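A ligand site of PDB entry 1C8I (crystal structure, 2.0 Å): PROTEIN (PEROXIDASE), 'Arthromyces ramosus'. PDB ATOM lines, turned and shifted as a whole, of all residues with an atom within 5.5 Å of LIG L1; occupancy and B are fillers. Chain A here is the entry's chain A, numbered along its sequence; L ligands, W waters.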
ATOM      1  N   SER A  45     -20.901   1.730 -40.592  1.00  0.00           N
ATOM      2  CA  SER A  45     -22.255   1.315 -40.285  1.00  0.00           C
ATOM      3  C   SER A  45     -22.603  -0.164 -40.608  1.00  0.00           C
ATOM      4  O   SER A  45     -23.216  -0.722 -39.697  1.00  0.00           O
ATOM      5  CB  SER A  45     -23.176   2.317 -41.034  1.00  0.00           C
ATOM      6  OG  SER A  45     -24.548   2.184 -40.742  1.00  0.00           O
ATOM      7  N   VAL A  47     -20.962  -2.973 -40.240  1.00  0.00           N
ATOM      8  CA  VAL A  47     -20.460  -3.762 -39.097  1.00  0.00           C
ATOM      9  C   VAL A  47     -21.313  -3.468 -37.855  1.00  0.00           C
ATOM     10  O   VAL A  47     -21.725  -4.387 -37.147  1.00  0.00           O
ATOM     11  CB  VAL A  47     -18.978  -3.405 -38.764  1.00  0.00           C
ATOM     12  CG1 VAL A  47     -18.546  -4.177 -37.538  1.00  0.00           C
ATOM     13  CG2 VAL A  47     -18.039  -3.727 -39.936  1.00  0.00           C
ATOM     14  N   ARG A  48     -21.614  -2.207 -37.553  1.00  0.00           N
ATOM     15  CA  ARG A  48     -22.384  -1.840 -36.367  1.00  0.00           C
ATOM     16  C   ARG A  48     -23.801  -2.394 -36.466  1.00  0.00           C
ATOM     17  O   ARG A  48     -24.335  -2.945 -35.497  1.00  0.00           O
ATOM     18  CB  ARG A  48     -22.378  -0.322 -36.224  1.00  0.00           C
ATOM     19  CG  ARG A  48     -20.969   0.260 -36.178  1.00  0.00           C
ATOM     20  CD  ARG A  48     -20.960   1.674 -35.613  1.00  0.00           C
ATOM     21  NE  ARG A  48     -21.846   2.538 -36.380  1.00  0.00           N
ATOM     22  CZ  ARG A  48     -21.412   3.387 -37.329  1.00  0.00           C
ATOM     23  NH1 ARG A  48     -22.327   4.148 -37.969  1.00  0.00           N
ATOM     24  NH2 ARG A  48     -20.120   3.467 -37.650  1.00  0.00           N
ATOM     25  N   LYS A  49     -24.415  -2.374 -37.649  1.00  0.00           N
ATOM     26  CA  LYS A  49     -25.737  -2.920 -37.879  1.00  0.00           C
ATOM     27  C   LYS A  49     -25.686  -4.438 -37.705  1.00  0.00           C
ATOM     28  O   LYS A  49     -26.573  -5.002 -37.052  1.00  0.00           O
ATOM     29  CB  LYS A  49     -26.198  -2.592 -39.291  1.00  0.00           C
ATOM     30  CG  LYS A  49     -26.436  -1.138 -39.627  1.00  0.00           C
ATOM     31  CD  LYS A  49     -27.578  -0.625 -38.775  1.00  0.00           C
ATOM     32  CE  LYS A  49     -28.042   0.720 -39.314  1.00  0.00           C
ATOM     33  NZ  LYS A  49     -29.142   1.260 -38.523  1.00  0.00           N
ATOM     34  N   LEU A  51     -23.697  -6.170 -35.763  1.00  0.00           N
ATOM     35  CA  LEU A  51     -23.561  -6.455 -34.343  1.00  0.00           C
ATOM     36  C   LEU A  51     -24.915  -6.348 -33.640  1.00  0.00           C
ATOM     37  O   LEU A  51     -25.193  -7.171 -32.753  1.00  0.00           O
ATOM     38  CB  LEU A  51     -22.541  -5.513 -33.711  1.00  0.00           C
ATOM     39  CG  LEU A  51     -21.065  -5.864 -33.960  1.00  0.00           C
ATOM     40  CD1 LEU A  51     -20.168  -4.747 -33.446  1.00  0.00           C
ATOM     41  CD2 LEU A  51     -20.722  -7.178 -33.259  1.00  0.00           C
ATOM     42  N   ARG A  52     -25.776  -5.364 -34.010  1.00  0.00           N
ATOM     43  CA  ARG A  52     -27.125  -5.276 -33.446  1.00  0.00           C
ATOM     44  C   ARG A  52     -27.877  -6.507 -33.886  1.00  0.00           C
ATOM     45  O   ARG A  52     -28.507  -7.166 -33.060  1.00  0.00           O
ATOM     46  CB  ARG A  52     -27.983  -4.130 -33.958  1.00  0.00           C
ATOM     47  CG  ARG A  52     -27.775  -2.802 -33.331  1.00  0.00           C
ATOM     48  CD  ARG A  52     -28.736  -1.753 -33.854  1.00  0.00           C
ATOM     49  NE  ARG A  52     -30.149  -1.913 -33.501  1.00  0.00           N
ATOM     50  CZ  ARG A  52     -31.097  -1.306 -34.250  1.00  0.00           C
ATOM     51  NH1 ARG A  52     -30.781  -0.550 -35.316  1.00  0.00           N
ATOM     52  NH2 ARG A  52     -32.388  -1.450 -33.964  1.00  0.00           N
ATOM     53  N   VAL A  54     -26.816  -9.673 -34.721  1.00  0.00           N
ATOM     54  CA  VAL A  54     -26.457 -10.940 -34.113  1.00  0.00           C
ATOM     55  C   VAL A  54     -27.039 -11.071 -32.704  1.00  0.00           C
ATOM     56  O   VAL A  54     -27.543 -12.130 -32.312  1.00  0.00           O
ATOM     57  CB  VAL A  54     -24.890 -11.050 -34.207  1.00  0.00           C
ATOM     58  CG1 VAL A  54     -24.133 -10.147 -33.223  1.00  0.00           C
ATOM     59  CG2 VAL A  54     -24.562 -12.499 -33.978  1.00  0.00           C
ATOM     60  N   PHE A  55     -27.066  -9.971 -31.942  1.00  0.00           N
ATOM     61  CA  PHE A  55     -27.638  -9.961 -30.594  1.00  0.00           C
ATOM     62  C   PHE A  55     -29.142 -10.184 -30.726  1.00  0.00           C
ATOM     63  O   PHE A  55     -29.652 -11.154 -30.168  1.00  0.00           O
ATOM     64  CB  PHE A  55     -27.352  -8.600 -29.889  1.00  0.00           C
ATOM     65  CG  PHE A  55     -28.020  -8.380 -28.524  1.00  0.00           C
ATOM     66  CD1 PHE A  55     -28.107  -9.404 -27.570  1.00  0.00           C
ATOM     67  CD2 PHE A  55     -28.572  -7.123 -28.219  1.00  0.00           C
ATOM     68  CE1 PHE A  55     -28.722  -9.177 -26.332  1.00  0.00           C
ATOM     69  CE2 PHE A  55     -29.180  -6.906 -26.989  1.00  0.00           C
ATOM     70  CZ  PHE A  55     -29.259  -7.925 -26.045  1.00  0.00           C
ATOM     71  N   PRO A 154     -33.941  -6.879 -24.762  1.00  0.00           N
ATOM     72  CA  PRO A 154     -33.822  -5.768 -23.796  1.00  0.00           C
ATOM     73  C   PRO A 154     -33.898  -4.403 -24.467  1.00  0.00           C
ATOM     74  O   PRO A 154     -33.320  -4.175 -25.541  1.00  0.00           O
ATOM     75  CB  PRO A 154     -32.490  -5.969 -23.132  1.00  0.00           C
ATOM     76  CG  PRO A 154     -32.257  -7.437 -23.229  1.00  0.00           C
ATOM     77  CD  PRO A 154     -32.824  -7.828 -24.608  1.00  0.00           C
ATOM     78  N   GLY A 155     -34.571  -3.456 -23.802  1.00  0.00           N
ATOM     79  CA  GLY A 155     -34.753  -2.111 -24.300  1.00  0.00           C
ATOM     80  C   GLY A 155     -33.957  -1.086 -23.492  1.00  0.00           C
ATOM     81  O   GLY A 155     -33.697  -1.298 -22.295  1.00  0.00           O
ATOM     82  N   PRO A 156     -33.589   0.064 -24.075  1.00  0.00           N
ATOM     83  CA  PRO A 156     -32.820   1.092 -23.424  1.00  0.00           C
ATOM     84  C   PRO A 156     -33.577   1.776 -22.281  1.00  0.00           C
ATOM     85  O   PRO A 156     -32.973   2.426 -21.440  1.00  0.00           O
ATOM     86  CB  PRO A 156     -32.430   2.027 -24.529  1.00  0.00           C
ATOM     87  CG  PRO A 156     -33.605   1.961 -25.471  1.00  0.00           C
ATOM     88  CD  PRO A 156     -33.958   0.471 -25.427  1.00  0.00           C
ATOM     89  N   ILE A 163     -33.347  -5.980 -17.400  1.00  0.00           N
ATOM     90  CA  ILE A 163     -32.301  -6.458 -18.326  1.00  0.00           C
ATOM     91  C   ILE A 163     -31.633  -7.712 -17.745  1.00  0.00           C
ATOM     92  O   ILE A 163     -31.585  -8.749 -18.426  1.00  0.00           O
ATOM     93  CB  ILE A 163     -31.270  -5.319 -18.548  1.00  0.00           C
ATOM     94  CG1 ILE A 163     -31.941  -4.158 -19.285  1.00  0.00           C
ATOM     95  CG2 ILE A 163     -30.070  -5.840 -19.326  1.00  0.00           C
ATOM     96  CD1 ILE A 163     -31.103  -2.857 -19.427  1.00  0.00           C
ATOM     97  N   MET A 167     -31.739 -11.328 -19.556  1.00  0.00           N
ATOM     98  CA  MET A 167     -30.455 -11.855 -19.949  1.00  0.00           C
ATOM     99  C   MET A 167     -30.138 -13.136 -19.208  1.00  0.00           C
ATOM    100  O   MET A 167     -29.590 -14.068 -19.797  1.00  0.00           O
ATOM    101  CB  MET A 167     -29.372 -10.801 -19.691  1.00  0.00           C
ATOM    102  CG  MET A 167     -29.425  -9.590 -20.627  1.00  0.00           C
ATOM    103  SD  MET A 167     -29.296 -10.015 -22.377  1.00  0.00           S
ATOM    104  CE  MET A 167     -27.547  -9.917 -22.641  1.00  0.00           C
ATOM    105  N   VAL A 177     -23.285  -9.974 -19.068  1.00  0.00           N
ATOM    106  CA  VAL A 177     -24.077  -8.873 -19.622  1.00  0.00           C
ATOM    107  C   VAL A 177     -23.110  -7.701 -19.787  1.00  0.00           C
ATOM    108  O   VAL A 177     -23.051  -7.093 -20.856  1.00  0.00           O
ATOM    109  CB  VAL A 177     -25.244  -8.449 -18.683  1.00  0.00           C
ATOM    110  CG1 VAL A 177     -25.970  -7.205 -19.239  1.00  0.00           C
ATOM    111  CG2 VAL A 177     -26.241  -9.585 -18.537  1.00  0.00           C
ATOM    112  N   LEU A 180     -20.631  -8.479 -22.765  1.00  0.00           N
ATOM    113  CA  LEU A 180     -21.335  -8.427 -24.039  1.00  0.00           C
ATOM    114  C   LEU A 180     -21.495  -6.973 -24.522  1.00  0.00           C
ATOM    115  O   LEU A 180     -21.366  -6.636 -25.712  1.00  0.00           O
ATOM    116  CB  LEU A 180     -22.648  -9.099 -23.765  1.00  0.00           C
ATOM    117  CG  LEU A 180     -23.163 -10.209 -24.643  1.00  0.00           C
ATOM    118  CD1 LEU A 180     -22.074 -11.037 -25.234  1.00  0.00           C
ATOM    119  CD2 LEU A 180     -24.082 -11.046 -23.801  1.00  0.00           C
ATOM    120  N   LEU A 181     -21.708  -6.037 -23.596  1.00  0.00           N
ATOM    121  CA  LEU A 181     -21.845  -4.634 -23.908  1.00  0.00           C
ATOM    122  C   LEU A 181     -20.581  -3.976 -24.411  1.00  0.00           C
ATOM    123  O   LEU A 181     -20.626  -2.773 -24.718  1.00  0.00           O
ATOM    124  CB  LEU A 181     -22.309  -3.854 -22.704  1.00  0.00           C
ATOM    125  CG  LEU A 181     -23.709  -3.266 -22.652  1.00  0.00           C
ATOM    126  CD1 LEU A 181     -24.423  -3.226 -23.995  1.00  0.00           C
ATOM    127  CD2 LEU A 181     -24.479  -4.150 -21.724  1.00  0.00           C
ATOM    128  N   ALA A 183     -19.510  -4.402 -27.249  1.00  0.00           N
ATOM    129  CA  ALA A 183     -19.860  -4.043 -28.613  1.00  0.00           C
ATOM    130  C   ALA A 183     -20.374  -2.597 -28.710  1.00  0.00           C
ATOM    131  O   ALA A 183     -20.342  -2.009 -29.791  1.00  0.00           O
ATOM    132  CB  ALA A 183     -20.913  -4.981 -29.126  1.00  0.00           C
ATOM    133  N   HIS A 184     -20.770  -1.905 -27.630  1.00  0.00           N
ATOM    134  CA  HIS A 184     -21.175  -0.520 -27.747  1.00  0.00           C
ATOM    135  C   HIS A 184     -19.967   0.412 -27.869  1.00  0.00           C
ATOM    136  O   HIS A 184     -20.084   1.639 -27.937  1.00  0.00           O
ATOM    137  CB  HIS A 184     -22.026  -0.096 -26.547  1.00  0.00           C
ATOM    138  CG  HIS A 184     -23.505  -0.468 -26.605  1.00  0.00           C
ATOM    139  ND1 HIS A 184     -24.473   0.074 -25.791  1.00  0.00           N
ATOM    140  CD2 HIS A 184     -24.094  -1.325 -27.538  1.00  0.00           C
ATOM    141  CE1 HIS A 184     -25.634  -0.420 -26.251  1.00  0.00           C
ATOM    142  NE2 HIS A 184     -25.457  -1.214 -27.255  1.00  0.00           N
ATOM    143  N   LEU A 186     -18.289   0.157 -30.528  1.00  0.00           N
ATOM    144  CA  LEU A 186     -18.281   0.288 -31.979  1.00  0.00           C
ATOM    145  C   LEU A 186     -19.731   0.640 -32.256  1.00  0.00           C
ATOM    146  O   LEU A 186     -20.447  -0.064 -32.962  1.00  0.00           O
ATOM    147  CB  LEU A 186     -17.899  -1.083 -32.509  1.00  0.00           C
ATOM    148  CG  LEU A 186     -16.575  -1.495 -33.159  1.00  0.00           C
ATOM    149  CD1 LEU A 186     -15.440  -0.595 -32.796  1.00  0.00           C
ATOM    150  CD2 LEU A 186     -16.336  -2.916 -32.761  1.00  0.00           C
ATOM    151  N   ALA A 187     -20.224   1.755 -31.738  1.00  0.00           N
ATOM    152  CA  ALA A 187     -21.646   2.013 -31.839  1.00  0.00           C
ATOM    153  C   ALA A 187     -22.101   3.438 -31.933  1.00  0.00           C
ATOM    154  O   ALA A 187     -21.425   4.347 -31.446  1.00  0.00           O
ATOM    155  CB  ALA A 187     -22.335   1.419 -30.621  1.00  0.00           C
ATOM    156  N   SER A 188     -23.269   3.632 -32.523  1.00  0.00           N
ATOM    157  CA  SER A 188     -23.876   4.942 -32.559  1.00  0.00           C
ATOM    158  C   SER A 188     -25.375   4.659 -32.424  1.00  0.00           C
ATOM    159  O   SER A 188     -25.800   3.503 -32.188  1.00  0.00           O
ATOM    160  CB  SER A 188     -23.584   5.638 -33.890  1.00  0.00           C
ATOM    161  OG  SER A 188     -24.237   5.071 -35.027  1.00  0.00           O
ATOM    162  N   GLN A 189     -26.208   5.693 -32.461  1.00  0.00           N
ATOM    163  CA  GLN A 189     -27.649   5.444 -32.495  1.00  0.00           C
ATOM    164  C   GLN A 189     -28.184   6.203 -33.706  1.00  0.00           C
ATOM    165  O   GLN A 189     -27.641   7.255 -34.107  1.00  0.00           O
ATOM    166  CB  GLN A 189     -28.316   5.955 -31.203  1.00  0.00           C
ATOM    167  CG  GLN A 189     -28.189   7.465 -30.907  1.00  0.00           C
ATOM    168  CD  GLN A 189     -29.189   8.376 -31.613  1.00  0.00           C
ATOM    169  OE1 GLN A 189     -30.286   7.948 -31.945  1.00  0.00           O
ATOM    170  NE2 GLN A 189     -28.898   9.645 -31.837  1.00  0.00           N
ATOM    171  N   GLU A 190     -29.273   5.757 -34.289  1.00  0.00           N
ATOM    172  CA  GLU A 190     -29.883   6.447 -35.417  1.00  0.00           C
ATOM    173  C   GLU A 190     -31.324   6.797 -35.111  1.00  0.00           C
ATOM    174  O   GLU A 190     -31.813   7.878 -35.479  1.00  0.00           O
ATOM    175  CB  GLU A 190     -29.879   5.602 -36.663  1.00  0.00           C
ATOM    176  CG  GLU A 190     -28.455   5.371 -37.204  1.00  0.00           C
ATOM    177  CD  GLU A 190     -28.353   4.568 -38.505  1.00  0.00           C
ATOM    178  OE1 GLU A 190     -29.347   4.042 -38.984  1.00  0.00           O
ATOM    179  OE2 GLU A 190     -27.263   4.466 -39.048  1.00  0.00           O
ATOM    180  N   GLY A 191     -31.999   5.907 -34.386  1.00  0.00           N
ATOM    181  CA  GLY A 191     -33.402   6.076 -34.094  1.00  0.00           C
ATOM    182  C   GLY A 191     -33.785   6.505 -32.697  1.00  0.00           C
ATOM    183  O   GLY A 191     -34.980   6.558 -32.414  1.00  0.00           O
ATOM    184  N   LEU A 192     -32.879   6.765 -31.754  1.00  0.00           N
ATOM    185  CA  LEU A 192     -33.280   7.183 -30.425  1.00  0.00           C
ATOM    186  C   LEU A 192     -33.407   8.704 -30.401  1.00  0.00           C
ATOM    187  O   LEU A 192     -34.243   9.286 -29.711  1.00  0.00           O
ATOM    188  CB  LEU A 192     -32.207   6.623 -29.495  1.00  0.00           C
ATOM    189  CG  LEU A 192     -32.449   5.449 -28.558  1.00  0.00           C
ATOM    190  CD1 LEU A 192     -33.463   4.454 -29.081  1.00  0.00           C
ATOM    191  CD2 LEU A 192     -31.095   4.855 -28.286  1.00  0.00           C
ATOM    192  N   LEU A 201     -21.504   6.347 -29.292  1.00  0.00           N
ATOM    193  CA  LEU A 201     -21.655   5.994 -27.887  1.00  0.00           C
ATOM    194  C   LEU A 201     -20.287   6.096 -27.203  1.00  0.00           C
ATOM    195  O   LEU A 201     -20.241   6.094 -25.964  1.00  0.00           O
ATOM    196  CB  LEU A 201     -22.265   4.588 -27.800  1.00  0.00           C
ATOM    197  CG  LEU A 201     -23.809   4.476 -27.671  1.00  0.00           C
ATOM    198  CD1 LEU A 201     -24.570   5.415 -28.573  1.00  0.00           C
ATOM    199  CD2 LEU A 201     -24.157   3.049 -28.030  1.00  0.00           C
ATOM    200  N   MET A 243     -27.050   6.530 -23.562  1.00  0.00           N
ATOM    201  CA  MET A 243     -28.268   5.730 -23.443  1.00  0.00           C
ATOM    202  C   MET A 243     -28.508   5.398 -21.950  1.00  0.00           C
ATOM    203  O   MET A 243     -27.570   5.096 -21.200  1.00  0.00           O
ATOM    204  CB  MET A 243     -28.027   4.498 -24.304  1.00  0.00           C
ATOM    205  CG  MET A 243     -29.210   3.506 -24.254  1.00  0.00           C
ATOM    206  SD  MET A 243     -28.780   2.070 -25.262  1.00  0.00           S
ATOM    207  CE  MET A 243     -27.647   2.773 -26.366  1.00  0.00           C
ATOM    208  N   SER A 245     -29.929   2.733 -20.209  1.00  0.00           N
ATOM    209  CA  SER A 245     -29.504   1.438 -19.740  1.00  0.00           C
ATOM    210  C   SER A 245     -27.997   1.373 -19.559  1.00  0.00           C
ATOM    211  O   SER A 245     -27.560   0.783 -18.561  1.00  0.00           O
ATOM    212  CB  SER A 245     -29.993   0.393 -20.725  1.00  0.00           C
ATOM    213  OG  SER A 245     -29.622   0.709 -22.059  1.00  0.00           O
ATOM    214  N   LEU A 249     -26.445   0.674 -15.932  1.00  0.00           N
ATOM    215  CA  LEU A 249     -25.601  -0.503 -15.752  1.00  0.00           C
ATOM    216  C   LEU A 249     -24.224  -0.126 -15.267  1.00  0.00           C
ATOM    217  O   LEU A 249     -23.655  -0.839 -14.450  1.00  0.00           O
ATOM    218  CB  LEU A 249     -25.472  -1.304 -17.068  1.00  0.00           C
ATOM    219  CG  LEU A 249     -26.751  -2.025 -17.506  1.00  0.00           C
ATOM    220  CD1 LEU A 249     -26.666  -2.398 -18.963  1.00  0.00           C
ATOM    221  CD2 LEU A 249     -26.955  -3.245 -16.632  1.00  0.00           C
ATOM    222  N   TYR A 273     -15.126 -10.446 -23.878  1.00  0.00           N
ATOM    223  CA  TYR A 273     -16.086 -10.295 -24.949  1.00  0.00           C
ATOM    224  C   TYR A 273     -16.085 -11.507 -25.865  1.00  0.00           C
ATOM    225  O   TYR A 273     -17.152 -12.016 -26.186  1.00  0.00           O
ATOM    226  CB  TYR A 273     -15.750  -9.002 -25.722  1.00  0.00           C
ATOM    227  CG  TYR A 273     -16.674  -8.769 -26.910  1.00  0.00           C
ATOM    228  CD1 TYR A 273     -18.004  -8.319 -26.731  1.00  0.00           C
ATOM    229  CD2 TYR A 273     -16.184  -9.046 -28.196  1.00  0.00           C
ATOM    230  CE1 TYR A 273     -18.835  -8.142 -27.848  1.00  0.00           C
ATOM    231  CE2 TYR A 273     -17.000  -8.861 -29.296  1.00  0.00           C
ATOM    232  CZ  TYR A 273     -18.321  -8.407 -29.127  1.00  0.00           C
ATOM    233  OH  TYR A 273     -19.075  -8.185 -30.257  1.00  0.00           O
ATOM    234  N   MET A 277     -19.397 -13.825 -26.472  1.00  0.00           N
ATOM    235  CA  MET A 277     -19.927 -13.983 -27.821  1.00  0.00           C
ATOM    236  C   MET A 277     -19.933 -15.433 -28.263  1.00  0.00           C
ATOM    237  O   MET A 277     -20.869 -15.803 -28.996  1.00  0.00           O
ATOM    238  CB  MET A 277     -19.111 -13.214 -28.863  1.00  0.00           C
ATOM    239  CG  MET A 277     -19.334 -11.728 -28.778  1.00  0.00           C
ATOM    240  SD  MET A 277     -21.005 -11.199 -29.273  1.00  0.00           S
ATOM    241  CE  MET A 277     -20.759 -11.177 -31.032  1.00  0.00           C
ATOM    242  N   MET A 280     -23.110 -16.762 -26.788  1.00  0.00           N
ATOM    243  CA  MET A 280     -24.269 -16.229 -27.453  1.00  0.00           C
ATOM    244  C   MET A 280     -24.466 -16.840 -28.826  1.00  0.00           C
ATOM    245  O   MET A 280     -25.597 -17.098 -29.204  1.00  0.00           O
ATOM    246  CB  MET A 280     -24.134 -14.713 -27.589  1.00  0.00           C
ATOM    247  CG  MET A 280     -25.459 -14.178 -28.083  1.00  0.00           C
ATOM    248  SD  MET A 280     -25.657 -12.408 -28.055  1.00  0.00           S
ATOM    249  CE  MET A 280     -24.606 -12.138 -29.442  1.00  0.00           C
HETATM  250  C1  LIG L   1     -26.923   0.216 -30.666  1.00  0.00           C
HETATM  251  C2  LIG L   1     -29.663  -1.011 -26.873  1.00  0.00           C
HETATM  252  C3  LIG L   1     -26.765  -4.772 -26.035  1.00  0.00           C
HETATM  253  C4  LIG L   1     -24.555  -3.965 -30.197  1.00  0.00           C
HETATM  254  C5  LIG L   1     -27.930   0.203 -29.706  1.00  0.00           C
HETATM  255  C6  LIG L   1     -29.086   1.075 -29.711  1.00  0.00           C
HETATM  256  C7  LIG L   1     -29.893   0.684 -28.691  1.00  0.00           C
HETATM  257  C8  LIG L   1     -29.225  -0.407 -28.053  1.00  0.00           C
HETATM  258  C9  LIG L   1     -31.253   1.238 -28.283  1.00  0.00           C
HETATM  259  C10 LIG L   1     -29.321   2.181 -30.715  1.00  0.00           C
HETATM  260  C11 LIG L   1     -29.993   1.712 -32.002  1.00  0.00           C
HETATM  261  C12 LIG L   1     -30.364   2.880 -32.881  1.00  0.00           C
HETATM  262  O1  LIG L   1     -29.804   3.022 -33.967  1.00  0.00           O
HETATM  263  O2  LIG L   1     -31.176   3.704 -32.477  1.00  0.00           O
HETATM  264  C13 LIG L   1     -29.011  -2.046 -26.216  1.00  0.00           C
HETATM  265  C14 LIG L   1     -29.433  -2.615 -24.950  1.00  0.00           C
HETATM  266  C15 LIG L   1     -28.621  -3.690 -24.716  1.00  0.00           C
HETATM  267  C16 LIG L   1     -27.665  -3.717 -25.811  1.00  0.00           C
HETATM  268  C17 LIG L   1     -30.563  -2.122 -24.039  1.00  0.00           C
HETATM  269  C18 LIG L   1     -28.775  -4.663 -23.729  1.00  0.00           C
HETATM  270  C19 LIG L   1     -28.176  -4.593 -22.415  1.00  0.00           C
HETATM  271  C20 LIG L   1     -25.972  -4.933 -27.147  1.00  0.00           C
HETATM  272  C21 LIG L   1     -25.188  -6.124 -27.406  1.00  0.00           C
HETATM  273  C22 LIG L   1     -24.616  -5.952 -28.633  1.00  0.00           C
HETATM  274  C23 LIG L   1     -25.024  -4.610 -29.069  1.00  0.00           C
HETATM  275  C24 LIG L   1     -25.094  -7.296 -26.421  1.00  0.00           C
HETATM  276  C25 LIG L   1     -23.899  -6.847 -29.452  1.00  0.00           C
HETATM  277  C26 LIG L   1     -22.931  -7.842 -29.066  1.00  0.00           C
HETATM  278  C27 LIG L   1     -24.933  -2.699 -30.630  1.00  0.00           C
HETATM  279  C28 LIG L   1     -24.260  -1.969 -31.671  1.00  0.00           C
HETATM  280  C29 LIG L   1     -24.938  -0.805 -31.806  1.00  0.00           C
HETATM  281  C30 LIG L   1     -25.975  -0.794 -30.812  1.00  0.00           C
HETATM  282  C31 LIG L   1     -22.951  -2.375 -32.340  1.00  0.00           C
HETATM  283  C32 LIG L   1     -24.667   0.304 -32.793  1.00  0.00           C
HETATM  284  C33 LIG L   1     -25.529   0.257 -34.046  1.00  0.00           C
HETATM  285  C34 LIG L   1     -25.226   1.370 -35.035  1.00  0.00           C
HETATM  286  O3  LIG L   1     -25.930   1.464 -36.041  1.00  0.00           O
HETATM  287  O4  LIG L   1     -24.324   2.157 -34.814  1.00  0.00           O
HETATM  288  N1  LIG L   1     -28.044  -0.743 -28.705  1.00  0.00           N
HETATM  289  N2  LIG L   1     -27.890  -2.695 -26.716  1.00  0.00           N
HETATM  290  N3  LIG L   1     -25.882  -4.019 -28.181  1.00  0.00           N
HETATM  291  N4  LIG L   1     -25.921  -1.937 -30.050  1.00  0.00           N
HETATM  292 FE1  LIG L   1     -26.860  -2.283 -28.371  1.00  0.00          FE
HETATM  293  N1  LG2 L   2     -28.141  -3.990 -30.232  1.00  0.00           N
HETATM  294  O1  LG2 L   2     -29.187  -3.480 -29.370  1.00  0.00           O
HETATM  295  O   HOH W   1     -28.723   1.229 -35.678  1.00  0.00           O
HETATM  296  O   HOH W   2     -24.987   2.895 -38.083  1.00  0.00           O
HETATM  297  O   HOH W   3     -27.531  -1.100 -22.556  1.00  0.00           O
HETATM  298  O   HOH W   4     -33.619   2.602 -31.696  1.00  0.00           O
HETATM  299  O   HOH W   5     -31.834   2.403 -36.111  1.00  0.00           O
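The backbone NH (N) of Gly 191 lies within hydrogen-bond range of an oxygen (O2) of LIG L1 (3.0 Å).
NH1 of Arg 52 lies within salt-bridge range of O1 of LIG L1, 3.9 Å away.
N of Ser 188 is in hydrogen-bond range of O4 of LIG L1 (2.9 Å).
An oxygen (O1) of LIG L1 lies within hydrogen-bond range of the backbone NH (N) of Glu 190, 2.8 Å away.
The side-chain hydroxyl of Ser 188 sits at hydrogen-bond distance from an oxygen (O4) of LIG L1 (2.9 Å).
The guanidinium group (NE) of Arg 48 is in salt-bridge range of an oxygen (O4) of LIG L1, 3.0 Å away.
An iron atom (FE1) of LIG L1 is bound by a ring nitrogen (NE2) of His 184, 2.1 Å away.
The backbone NH (N) of Ser 245 lies within hydrogen-bond range of the backbone carbonyl oxygen (O) of Pro 156.
The side-chain carboxylate (OE1) of Glu 190 lies within salt-bridge range of the side-chain amino group (NZ) of Lys 49 (2.8 Å).
N of Leu 192 sits at hydrogen-bond distance from OE1 of Gln 189 (2.9 Å).
The side-chain hydroxyl of Ser 245 sits close to the side-chain sulfur of Met 243 (3.6 Å).
The backbone NH (N) of Leu 201 sits at hydrogen-bond distance from the backbone carbonyl oxygen (O) of Ala 187 (2.9 Å).
SD of Met 277 sits close to OH of Tyr 273, at 3.7 Å.
Merely in contact with LIG L1: Lys 49 (3.8 Å), Leu 51 (3.4 Å), Phe 55 (3.4 Å), Pro 154 (3.8 Å), Gly 155 (3.6 Å), Pro 156 (3.7 Å), Ile 163 (3.8 Å), Leu 180 (3.9 Å), Leu 181 (3.5 Å), Ala 183 (3.5 Å), Leu 186 (3.5 Å), Ala 187 (3.4 Å), Gln 189 (3.6 Å), Leu 192 (3.6 Å), Met 243 (3.6 Å), Ser 245 (3.6 Å) and Met 277 (3.9 Å).
Hydrophobic or aromatic side chains that line LIG L1: Leu 51, Phe 55, Pro 154, Pro 156, Ile 163, Leu 180, Leu 181, Ala 183, His 184, Ala 187, Leu 192, Met 243 and Met 277.
Water W2 lies within hydrogen-bond range of an oxygen (O3) of LIG L1 (2.7 Å), the side-chain hydroxyl of Ser 45 (2.8 Å), the side-chain carboxylate of Glu 190 (2.9 Å) and the guanidinium group of Arg 48 (2.9 Å).
Water W1 lies within hydrogen-bond range of an oxygen (O1) of LIG L1, the guanidinium group of Arg 52 and the side-chain amino group of Lys 49.
Water W5 lies within hydrogen-bond range of O1 of LIG L1 (3.0 Å) and NH1 of Arg 52 (3.2 Å).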
